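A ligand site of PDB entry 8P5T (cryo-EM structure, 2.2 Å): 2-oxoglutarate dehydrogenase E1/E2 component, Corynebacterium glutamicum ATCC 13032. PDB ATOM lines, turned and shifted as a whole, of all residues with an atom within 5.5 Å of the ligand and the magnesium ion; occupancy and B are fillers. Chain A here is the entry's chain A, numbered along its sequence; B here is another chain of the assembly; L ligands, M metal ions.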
ATOM      1  N   HIS A 545     -11.753   1.993 -27.460  1.00  0.00           N
ATOM      2  CA  HIS A 545     -10.744   2.312 -26.454  1.00  0.00           C
ATOM      3  C   HIS A 545     -10.480   1.207 -25.437  1.00  0.00           C
ATOM      4  O   HIS A 545      -9.363   1.074 -24.961  1.00  0.00           O
ATOM      5  CB  HIS A 545     -11.191   3.566 -25.691  1.00  0.00           C
ATOM      6  CG  HIS A 545     -12.556   3.450 -25.100  1.00  0.00           C
ATOM      7  ND1 HIS A 545     -13.719   3.596 -25.835  1.00  0.00           N
ATOM      8  CD2 HIS A 545     -12.962   3.167 -23.853  1.00  0.00           C
ATOM      9  CE1 HIS A 545     -14.771   3.409 -25.046  1.00  0.00           C
ATOM     10  NE2 HIS A 545     -14.333   3.136 -23.846  1.00  0.00           N
ATOM     11  N   ARG A 546     -11.508   0.438 -25.075  1.00  0.00           N
ATOM     12  CA  ARG A 546     -11.455  -0.490 -23.949  1.00  0.00           C
ATOM     13  C   ARG A 546     -10.529  -1.659 -24.248  1.00  0.00           C
ATOM     14  O   ARG A 546     -10.895  -2.590 -24.965  1.00  0.00           O
ATOM     15  CB  ARG A 546     -12.875  -0.995 -23.686  1.00  0.00           C
ATOM     16  CG  ARG A 546     -13.062  -2.000 -22.553  1.00  0.00           C
ATOM     17  CD  ARG A 546     -12.795  -1.428 -21.190  1.00  0.00           C
ATOM     18  NE  ARG A 546     -13.674  -0.339 -20.841  1.00  0.00           N
ATOM     19  CZ  ARG A 546     -13.364   0.608 -19.960  1.00  0.00           C
ATOM     20  NH1 ARG A 546     -12.232   0.561 -19.301  1.00  0.00           N
ATOM     21  NH2 ARG A 546     -14.174   1.612 -19.761  1.00  0.00           N
ATOM     22  N   SER A 610     -12.466   9.146 -31.872  1.00  0.00           N
ATOM     23  CA  SER A 610     -13.175   8.936 -30.630  1.00  0.00           C
ATOM     24  C   SER A 610     -14.650   8.658 -30.862  1.00  0.00           C
ATOM     25  O   SER A 610     -15.279   7.983 -30.061  1.00  0.00           O
ATOM     26  CB  SER A 610     -13.017  10.114 -29.730  1.00  0.00           C
ATOM     27  OG  SER A 610     -11.679  10.195 -29.242  1.00  0.00           O
ATOM     28  N   HIS A 611     -15.209   9.177 -31.960  1.00  0.00           N
ATOM     29  CA  HIS A 611     -16.589   8.951 -32.321  1.00  0.00           C
ATOM     30  C   HIS A 611     -16.838   7.457 -32.448  1.00  0.00           C
ATOM     31  O   HIS A 611     -16.236   6.809 -33.299  1.00  0.00           O
ATOM     32  CB  HIS A 611     -16.912   9.628 -33.640  1.00  0.00           C
ATOM     33  CG  HIS A 611     -16.830  11.112 -33.610  1.00  0.00           C
ATOM     34  ND1 HIS A 611     -15.688  11.800 -33.288  1.00  0.00           N
ATOM     35  CD2 HIS A 611     -17.731  12.023 -33.905  1.00  0.00           C
ATOM     36  CE1 HIS A 611     -15.944  13.095 -33.362  1.00  0.00           C
ATOM     37  NE2 HIS A 611     -17.171  13.245 -33.733  1.00  0.00           N
ATOM     38  N   LEU A 612     -17.732   6.922 -31.626  1.00  0.00           N
ATOM     39  CA  LEU A 612     -17.938   5.488 -31.532  1.00  0.00           C
ATOM     40  C   LEU A 612     -18.665   4.969 -32.761  1.00  0.00           C
ATOM     41  O   LEU A 612     -19.585   5.613 -33.251  1.00  0.00           O
ATOM     42  CB  LEU A 612     -18.746   5.207 -30.261  1.00  0.00           C
ATOM     43  CG  LEU A 612     -17.995   5.408 -28.942  1.00  0.00           C
ATOM     44  CD1 LEU A 612     -18.945   5.434 -27.756  1.00  0.00           C
ATOM     45  CD2 LEU A 612     -16.969   4.320 -28.726  1.00  0.00           C
ATOM     46  N   GLY A 646     -18.883  -2.091 -27.668  1.00  0.00           N
ATOM     47  CA  GLY A 646     -19.379  -2.005 -26.307  1.00  0.00           C
ATOM     48  C   GLY A 646     -20.894  -2.041 -26.269  1.00  0.00           C
ATOM     49  O   GLY A 646     -21.540  -1.768 -27.281  1.00  0.00           O
ATOM     50  N   ASP A 647     -21.478  -2.337 -25.106  1.00  0.00           N
ATOM     51  CA  ASP A 647     -22.885  -2.678 -24.996  1.00  0.00           C
ATOM     52  C   ASP A 647     -23.766  -1.457 -25.216  1.00  0.00           C
ATOM     53  O   ASP A 647     -24.740  -1.537 -25.967  1.00  0.00           O
ATOM     54  CB  ASP A 647     -23.194  -3.397 -23.682  1.00  0.00           C
ATOM     55  CG  ASP A 647     -22.689  -2.722 -22.422  1.00  0.00           C
ATOM     56  OD1 ASP A 647     -22.119  -1.618 -22.527  1.00  0.00           O
ATOM     57  OD2 ASP A 647     -22.866  -3.312 -21.325  1.00  0.00           O
ATOM     58  N   ALA A 648     -23.437  -0.317 -24.606  1.00  0.00           N
ATOM     59  CA  ALA A 648     -24.224   0.893 -24.773  1.00  0.00           C
ATOM     60  C   ALA A 648     -24.177   1.397 -26.203  1.00  0.00           C
ATOM     61  O   ALA A 648     -25.201   1.784 -26.756  1.00  0.00           O
ATOM     62  CB  ALA A 648     -23.730   1.944 -23.838  1.00  0.00           C
ATOM     63  N   ALA A 649     -23.003   1.369 -26.830  1.00  0.00           N
ATOM     64  CA  ALA A 649     -22.846   1.884 -28.172  1.00  0.00           C
ATOM     65  C   ALA A 649     -23.551   1.004 -29.193  1.00  0.00           C
ATOM     66  O   ALA A 649     -24.094   1.518 -30.171  1.00  0.00           O
ATOM     67  CB  ALA A 649     -21.396   1.993 -28.492  1.00  0.00           C
ATOM     68  N   PHE A 650     -23.565  -0.306 -28.989  1.00  0.00           N
ATOM     69  CA  PHE A 650     -24.119  -1.221 -29.946  1.00  0.00           C
ATOM     70  C   PHE A 650     -25.631  -1.072 -30.041  1.00  0.00           C
ATOM     71  O   PHE A 650     -26.189  -1.213 -31.120  1.00  0.00           O
ATOM     72  CB  PHE A 650     -23.757  -2.648 -29.563  1.00  0.00           C
ATOM     73  CG  PHE A 650     -24.045  -3.705 -30.602  1.00  0.00           C
ATOM     74  CD1 PHE A 650     -23.125  -4.019 -31.566  1.00  0.00           C
ATOM     75  CD2 PHE A 650     -25.242  -4.380 -30.604  1.00  0.00           C
ATOM     76  CE1 PHE A 650     -23.392  -4.998 -32.505  1.00  0.00           C
ATOM     77  CE2 PHE A 650     -25.505  -5.349 -31.545  1.00  0.00           C
ATOM     78  CZ  PHE A 650     -24.581  -5.662 -32.490  1.00  0.00           C
ATOM     79  N   LEU A 653     -26.457   3.573 -31.182  1.00  0.00           N
ATOM     80  CA  LEU A 653     -26.109   4.271 -32.399  1.00  0.00           C
ATOM     81  C   LEU A 653     -26.661   3.529 -33.601  1.00  0.00           C
ATOM     82  O   LEU A 653     -26.646   2.304 -33.628  1.00  0.00           O
ATOM     83  CB  LEU A 653     -24.590   4.390 -32.457  1.00  0.00           C
ATOM     84  CG  LEU A 653     -23.973   5.314 -31.422  1.00  0.00           C
ATOM     85  CD1 LEU A 653     -22.472   5.138 -31.373  1.00  0.00           C
ATOM     86  CD2 LEU A 653     -24.295   6.751 -31.722  1.00  0.00           C
ATOM     87  N   VAL A 678     -18.575  -6.617 -25.761  1.00  0.00           N
ATOM     88  CA  VAL A 678     -18.049  -6.674 -24.407  1.00  0.00           C
ATOM     89  C   VAL A 678     -19.080  -6.077 -23.470  1.00  0.00           C
ATOM     90  O   VAL A 678     -19.143  -4.879 -23.307  1.00  0.00           O
ATOM     91  CB  VAL A 678     -16.696  -5.970 -24.297  1.00  0.00           C
ATOM     92  CG1 VAL A 678     -16.085  -6.110 -22.932  1.00  0.00           C
ATOM     93  CG2 VAL A 678     -15.714  -6.460 -25.317  1.00  0.00           C
ATOM     94  N   ASN A 679     -19.873  -6.935 -22.840  1.00  0.00           N
ATOM     95  CA  ASN A 679     -21.029  -6.559 -22.059  1.00  0.00           C
ATOM     96  C   ASN A 679     -20.622  -6.505 -20.599  1.00  0.00           C
ATOM     97  O   ASN A 679     -20.639  -7.523 -19.912  1.00  0.00           O
ATOM     98  CB  ASN A 679     -22.146  -7.552 -22.332  1.00  0.00           C
ATOM     99  CG  ASN A 679     -23.448  -7.208 -21.660  1.00  0.00           C
ATOM    100  OD1 ASN A 679     -23.901  -6.064 -21.717  1.00  0.00           O
ATOM    101  ND2 ASN A 679     -24.060  -8.182 -21.016  1.00  0.00           N
ATOM    102  N   ASN A 680     -20.245  -5.315 -20.128  1.00  0.00           N
ATOM    103  CA  ASN A 680     -19.795  -5.121 -18.764  1.00  0.00           C
ATOM    104  C   ASN A 680     -20.835  -4.366 -17.955  1.00  0.00           C
ATOM    105  O   ASN A 680     -20.541  -3.847 -16.890  1.00  0.00           O
ATOM    106  CB  ASN A 680     -18.436  -4.448 -18.734  1.00  0.00           C
ATOM    107  CG  ASN A 680     -18.397  -3.090 -19.359  1.00  0.00           C
ATOM    108  OD1 ASN A 680     -19.431  -2.501 -19.613  1.00  0.00           O
ATOM    109  ND2 ASN A 680     -17.203  -2.573 -19.586  1.00  0.00           N
ATOM    110  N   GLN A 681     -22.047  -4.321 -18.472  1.00  0.00           N
ATOM    111  CA  GLN A 681     -23.241  -3.989 -17.719  1.00  0.00           C
ATOM    112  C   GLN A 681     -23.236  -2.541 -17.278  1.00  0.00           C
ATOM    113  O   GLN A 681     -23.851  -2.216 -16.277  1.00  0.00           O
ATOM    114  CB  GLN A 681     -23.376  -4.982 -16.578  1.00  0.00           C
ATOM    115  CG  GLN A 681     -23.337  -6.423 -17.050  1.00  0.00           C
ATOM    116  CD  GLN A 681     -23.542  -7.412 -15.935  1.00  0.00           C
ATOM    117  OE1 GLN A 681     -24.633  -7.530 -15.392  1.00  0.00           O
ATOM    118  NE2 GLN A 681     -22.489  -8.126 -15.589  1.00  0.00           N
ATOM    119  N   ILE A 682     -22.596  -1.651 -18.044  1.00  0.00           N
ATOM    120  CA  ILE A 682     -22.526  -0.250 -17.683  1.00  0.00           C
ATOM    121  C   ILE A 682     -21.983   0.571 -18.842  1.00  0.00           C
ATOM    122  O   ILE A 682     -21.140   0.123 -19.590  1.00  0.00           O
ATOM    123  CB  ILE A 682     -21.699  -0.069 -16.398  1.00  0.00           C
ATOM    124  CG1 ILE A 682     -21.852   1.342 -15.837  1.00  0.00           C
ATOM    125  CG2 ILE A 682     -20.250  -0.422 -16.617  1.00  0.00           C
ATOM    126  CD1 ILE A 682     -21.740   1.406 -14.347  1.00  0.00           C
ATOM    127  N   GLY A 683     -22.485   1.808 -18.939  1.00  0.00           N
ATOM    128  CA  GLY A 683     -22.076   2.783 -19.931  1.00  0.00           C
ATOM    129  C   GLY A 683     -20.905   3.608 -19.425  1.00  0.00           C
ATOM    130  O   GLY A 683     -19.771   3.128 -19.451  1.00  0.00           O
ATOM    131  N   PHE A 684     -21.172   4.832 -18.995  1.00  0.00           N
ATOM    132  CA  PHE A 684     -20.186   5.621 -18.271  1.00  0.00           C
ATOM    133  C   PHE A 684     -20.715   5.735 -16.845  1.00  0.00           C
ATOM    134  O   PHE A 684     -20.119   5.187 -15.916  1.00  0.00           O
ATOM    135  CB  PHE A 684     -19.958   6.929 -19.034  1.00  0.00           C
ATOM    136  CG  PHE A 684     -19.109   7.990 -18.392  1.00  0.00           C
ATOM    137  CD1 PHE A 684     -18.585   7.862 -17.113  1.00  0.00           C
ATOM    138  CD2 PHE A 684     -18.837   9.158 -19.078  1.00  0.00           C
ATOM    139  CE1 PHE A 684     -17.822   8.867 -16.549  1.00  0.00           C
ATOM    140  CE2 PHE A 684     -18.076  10.163 -18.524  1.00  0.00           C
ATOM    141  CZ  PHE A 684     -17.564  10.015 -17.261  1.00  0.00           C
ATOM    142  N   ARG A 745     -16.684  -4.264 -15.056  1.00  0.00           N
ATOM    143  CA  ARG A 745     -15.659  -3.223 -15.086  1.00  0.00           C
ATOM    144  C   ARG A 745     -15.174  -2.955 -13.666  1.00  0.00           C
ATOM    145  O   ARG A 745     -15.956  -2.499 -12.849  1.00  0.00           O
ATOM    146  CB  ARG A 745     -16.277  -1.967 -15.684  1.00  0.00           C
ATOM    147  CG  ARG A 745     -15.305  -0.873 -16.069  1.00  0.00           C
ATOM    148  CD  ARG A 745     -15.990   0.429 -16.381  1.00  0.00           C
ATOM    149  NE  ARG A 745     -16.567   1.014 -15.179  1.00  0.00           N
ATOM    150  CZ  ARG A 745     -17.477   1.970 -15.170  1.00  0.00           C
ATOM    151  NH1 ARG A 745     -17.884   2.526 -16.283  1.00  0.00           N
ATOM    152  NH2 ARG A 745     -17.984   2.375 -14.026  1.00  0.00           N
ATOM    153  N   HIS A 749     -14.865   4.551 -15.188  1.00  0.00           N
ATOM    154  CA  HIS A 749     -14.833   4.666 -16.625  1.00  0.00           C
ATOM    155  C   HIS A 749     -13.392   4.904 -17.049  1.00  0.00           C
ATOM    156  O   HIS A 749     -12.909   4.271 -17.989  1.00  0.00           O
ATOM    157  CB  HIS A 749     -15.746   5.792 -17.106  1.00  0.00           C
ATOM    158  CG  HIS A 749     -15.847   5.860 -18.592  1.00  0.00           C
ATOM    159  ND1 HIS A 749     -15.289   6.872 -19.332  1.00  0.00           N
ATOM    160  CD2 HIS A 749     -16.383   5.022 -19.458  1.00  0.00           C
ATOM    161  CE1 HIS A 749     -15.518   6.639 -20.605  1.00  0.00           C
ATOM    162  NE2 HIS A 749     -16.185   5.524 -20.715  1.00  0.00           N
ATOM    163  N   GLU B 903     -26.384  13.037 -22.202  1.00  0.00           N
ATOM    164  CA  GLU B 903     -25.604  11.901 -21.744  1.00  0.00           C
ATOM    165  C   GLU B 903     -24.929  12.217 -20.420  1.00  0.00           C
ATOM    166  O   GLU B 903     -24.080  13.102 -20.356  1.00  0.00           O
ATOM    167  CB  GLU B 903     -24.522  11.514 -22.745  1.00  0.00           C
ATOM    168  CG  GLU B 903     -25.053  10.831 -23.998  1.00  0.00           C
ATOM    169  CD  GLU B 903     -24.046  10.676 -25.131  1.00  0.00           C
ATOM    170  OE1 GLU B 903     -24.473  10.341 -26.259  1.00  0.00           O
ATOM    171  OE2 GLU B 903     -22.835  10.892 -24.877  1.00  0.00           O
ATOM    172  N   LEU B 949     -27.307   6.613 -25.876  1.00  0.00           N
ATOM    173  CA  LEU B 949     -26.112   7.072 -26.549  1.00  0.00           C
ATOM    174  C   LEU B 949     -26.442   7.375 -28.012  1.00  0.00           C
ATOM    175  O   LEU B 949     -26.172   6.571 -28.899  1.00  0.00           O
ATOM    176  CB  LEU B 949     -25.039   5.984 -26.395  1.00  0.00           C
ATOM    177  CG  LEU B 949     -23.598   6.477 -26.342  1.00  0.00           C
ATOM    178  CD1 LEU B 949     -22.671   5.353 -25.927  1.00  0.00           C
ATOM    179  CD2 LEU B 949     -23.153   7.025 -27.688  1.00  0.00           C
ATOM    180  N   GLU B 951     -26.980  11.088 -30.729  1.00  0.00           N
ATOM    181  CA  GLU B 951     -26.965  12.527 -30.906  1.00  0.00           C
ATOM    182  C   GLU B 951     -28.054  12.962 -31.871  1.00  0.00           C
ATOM    183  O   GLU B 951     -28.618  14.043 -31.722  1.00  0.00           O
ATOM    184  CB  GLU B 951     -25.588  12.996 -31.392  1.00  0.00           C
ATOM    185  CG  GLU B 951     -24.545  13.059 -30.295  1.00  0.00           C
ATOM    186  CD  GLU B 951     -23.825  11.771 -29.951  1.00  0.00           C
ATOM    187  OE1 GLU B 951     -24.107  10.737 -30.593  1.00  0.00           O
ATOM    188  OE2 GLU B 951     -22.970  11.808 -29.027  1.00  0.00           O
ATOM    189  N   GLN B 975     -21.980  15.629 -24.474  1.00  0.00           N
ATOM    190  CA  GLN B 975     -20.916  15.191 -23.584  1.00  0.00           C
ATOM    191  C   GLN B 975     -19.672  16.002 -23.853  1.00  0.00           C
ATOM    192  O   GLN B 975     -19.062  16.522 -22.938  1.00  0.00           O
ATOM    193  CB  GLN B 975     -20.700  13.687 -23.738  1.00  0.00           C
ATOM    194  CG  GLN B 975     -19.665  13.151 -22.790  1.00  0.00           C
ATOM    195  CD  GLN B 975     -19.961  11.742 -22.341  1.00  0.00           C
ATOM    196  OE1 GLN B 975     -19.237  10.809 -22.663  1.00  0.00           O
ATOM    197  NE2 GLN B 975     -21.003  11.596 -21.549  1.00  0.00           N
ATOM    198  N   PHE B 979     -19.075  16.072 -30.607  1.00  0.00           N
ATOM    199  CA  PHE B 979     -19.911  14.970 -31.042  1.00  0.00           C
ATOM    200  C   PHE B 979     -21.232  15.470 -31.616  1.00  0.00           C
ATOM    201  O   PHE B 979     -22.085  14.665 -31.955  1.00  0.00           O
ATOM    202  CB  PHE B 979     -20.123  14.018 -29.878  1.00  0.00           C
ATOM    203  CG  PHE B 979     -18.866  13.381 -29.347  1.00  0.00           C
ATOM    204  CD1 PHE B 979     -17.975  12.768 -30.191  1.00  0.00           C
ATOM    205  CD2 PHE B 979     -18.585  13.403 -28.001  1.00  0.00           C
ATOM    206  CE1 PHE B 979     -16.807  12.196 -29.711  1.00  0.00           C
ATOM    207  CE2 PHE B 979     -17.414  12.832 -27.511  1.00  0.00           C
ATOM    208  CZ  PHE B 979     -16.536  12.243 -28.375  1.00  0.00           C
HETATM  209  N1  LIG L   1     -20.999   9.724 -28.608  1.00  0.00           N
HETATM  210  C1  LIG L   1     -20.095   9.331 -29.498  1.00  0.00           C
HETATM  211  C2  LIG L   1     -20.548   9.195 -30.919  1.00  0.00           C
HETATM  212  N2  LIG L   1     -18.816   9.069 -29.228  1.00  0.00           N
HETATM  213  C3  LIG L   1     -18.414   9.198 -27.961  1.00  0.00           C
HETATM  214  N3  LIG L   1     -17.119   8.932 -27.725  1.00  0.00           N
HETATM  215  C4  LIG L   1     -19.295   9.595 -26.942  1.00  0.00           C
HETATM  216  C5  LIG L   1     -20.587   9.849 -27.341  1.00  0.00           C
HETATM  217  C6  LIG L   1     -18.877   9.743 -25.494  1.00  0.00           C
HETATM  218  N4  LIG L   1     -18.595   8.469 -24.822  1.00  0.00           N
HETATM  219  C7  LIG L   1     -17.349   7.974 -24.665  1.00  0.00           C
HETATM  220  S1  LIG L   1     -17.420   6.527 -23.889  1.00  0.00           S
HETATM  221  C8  LIG L   1     -19.027   6.479 -23.686  1.00  0.00           C
HETATM  222  C9  LIG L   1     -19.560   7.623 -24.250  1.00  0.00           C
HETATM  223  C10 LIG L   1     -21.022   7.971 -24.305  1.00  0.00           C
HETATM  224  C11 LIG L   1     -19.594   5.304 -22.989  1.00  0.00           C
HETATM  225  C12 LIG L   1     -19.503   4.088 -23.835  1.00  0.00           C
HETATM  226  O1  LIG L   1     -20.140   2.986 -23.160  1.00  0.00           O
HETATM  227  P1  LIG L   1     -19.866   1.506 -23.668  1.00  0.00           P
HETATM  228  O2  LIG L   1     -20.558   0.557 -22.762  1.00  0.00           O
HETATM  229  O3  LIG L   1     -20.145   1.430 -25.111  1.00  0.00           O
HETATM  230  O4  LIG L   1     -18.300   1.383 -23.381  1.00  0.00           O
HETATM  231  P2  LIG L   1     -17.415   0.787 -22.190  1.00  0.00           P
HETATM  232  O5  LIG L   1     -16.939   1.945 -21.428  1.00  0.00           O
HETATM  233  O6  LIG L   1     -18.362  -0.055 -21.447  1.00  0.00           O
HETATM  234  O7  LIG L   1     -16.319   0.012 -22.804  1.00  0.00           O
HETATM  235 MG    MG M   1     -20.173  -1.148 -21.223  1.00  0.00          MG
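O6 of the ligand binds the magnesium ion. The side-chain amide oxygen (OD1) of Asn 680 binds the magnesium ion. The backbone carbonyl oxygen (O) of Ile 682 binds the magnesium ion, 2.3 Å away. The magnesium ion is bound by O2 of the ligand, 2.3 Å away. OD1 of Asp 647 binds the magnesium ion (2.4 Å). The magnesium ion has five donor atoms within binding distance.
A sulfur (S1) of the ligand sits close to a ring nitrogen (NE2) of His 749 (3.6 Å). A nitrogen (N2) of the ligand lies within hydrogen-bond range of the backbone NH of Leu 612, at 3.4 Å. An oxygen (O3) of the ligand is in hydrogen-bond range of the backbone NH of Ala 649, at 3.3 Å. The side-chain carboxylate (OE2) of Glu 951 of chain B sits at hydrogen-bond distance from a nitrogen (N1) of the ligand (2.9 Å). NH2 of Arg 546 lies within salt-bridge range of O5 of the ligand, 3.2 Å away. A nitrogen (N3) of the ligand lies within hydrogen-bond range of the backbone carbonyl oxygen (O) of Ser 610 (3.1 Å).
The side-chain carboxylate of Asp 647 lies close to the side-chain amide oxygen of Asn 679, 3.0 Å away. The side-chain carboxylate (OD2) of Asp 647 lies within hydrogen-bond range of the backbone NH (N) of Gln 681 (3.1 Å). The backbone carbonyl oxygen (O) of His 749 is in hydrogen-bond range of the guanidinium group (NH2) of Arg 546 (3.4 Å).
Three residues have an atom within 4 Å of the magnesium ion: Asp 647, Asn 680 and Ile 682. The nearest printed residue that does not touch the magnesium ion is Gly 683 (4.4 Å).
The side-chain amide oxygen of Gln 975 of chain B lies close to a nitrogen (N4) of the ligand. Merely in contact with the ligand: His 545, His 611, Gly 646, Ala 648, Gly 683, Glu 903 of chain B, Leu 949 of chain B and Phe 979 of chain B. Hydrophobic or aromatic side chains that line the ligand: Leu 612, Ala 648, Ala 649, His 749, Leu 949 of chain B and Phe 979 of chain B. 18 residues have an atom within 4 Å of the ligand: His 545, Arg 546, Ser 610, His 611, Leu 612, Gly 646, Asp 647, Ala 648, Ala 649, Asn 680, Ile 682, Gly 683, His 749, Glu 903 of chain B, Leu 949 of chain B, Glu 951 of chain B, Gln 975 of chain B and Phe 979 of chain B. The nearest printed residue that does not touch the ligand is Phe 684 (4.3 Å).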
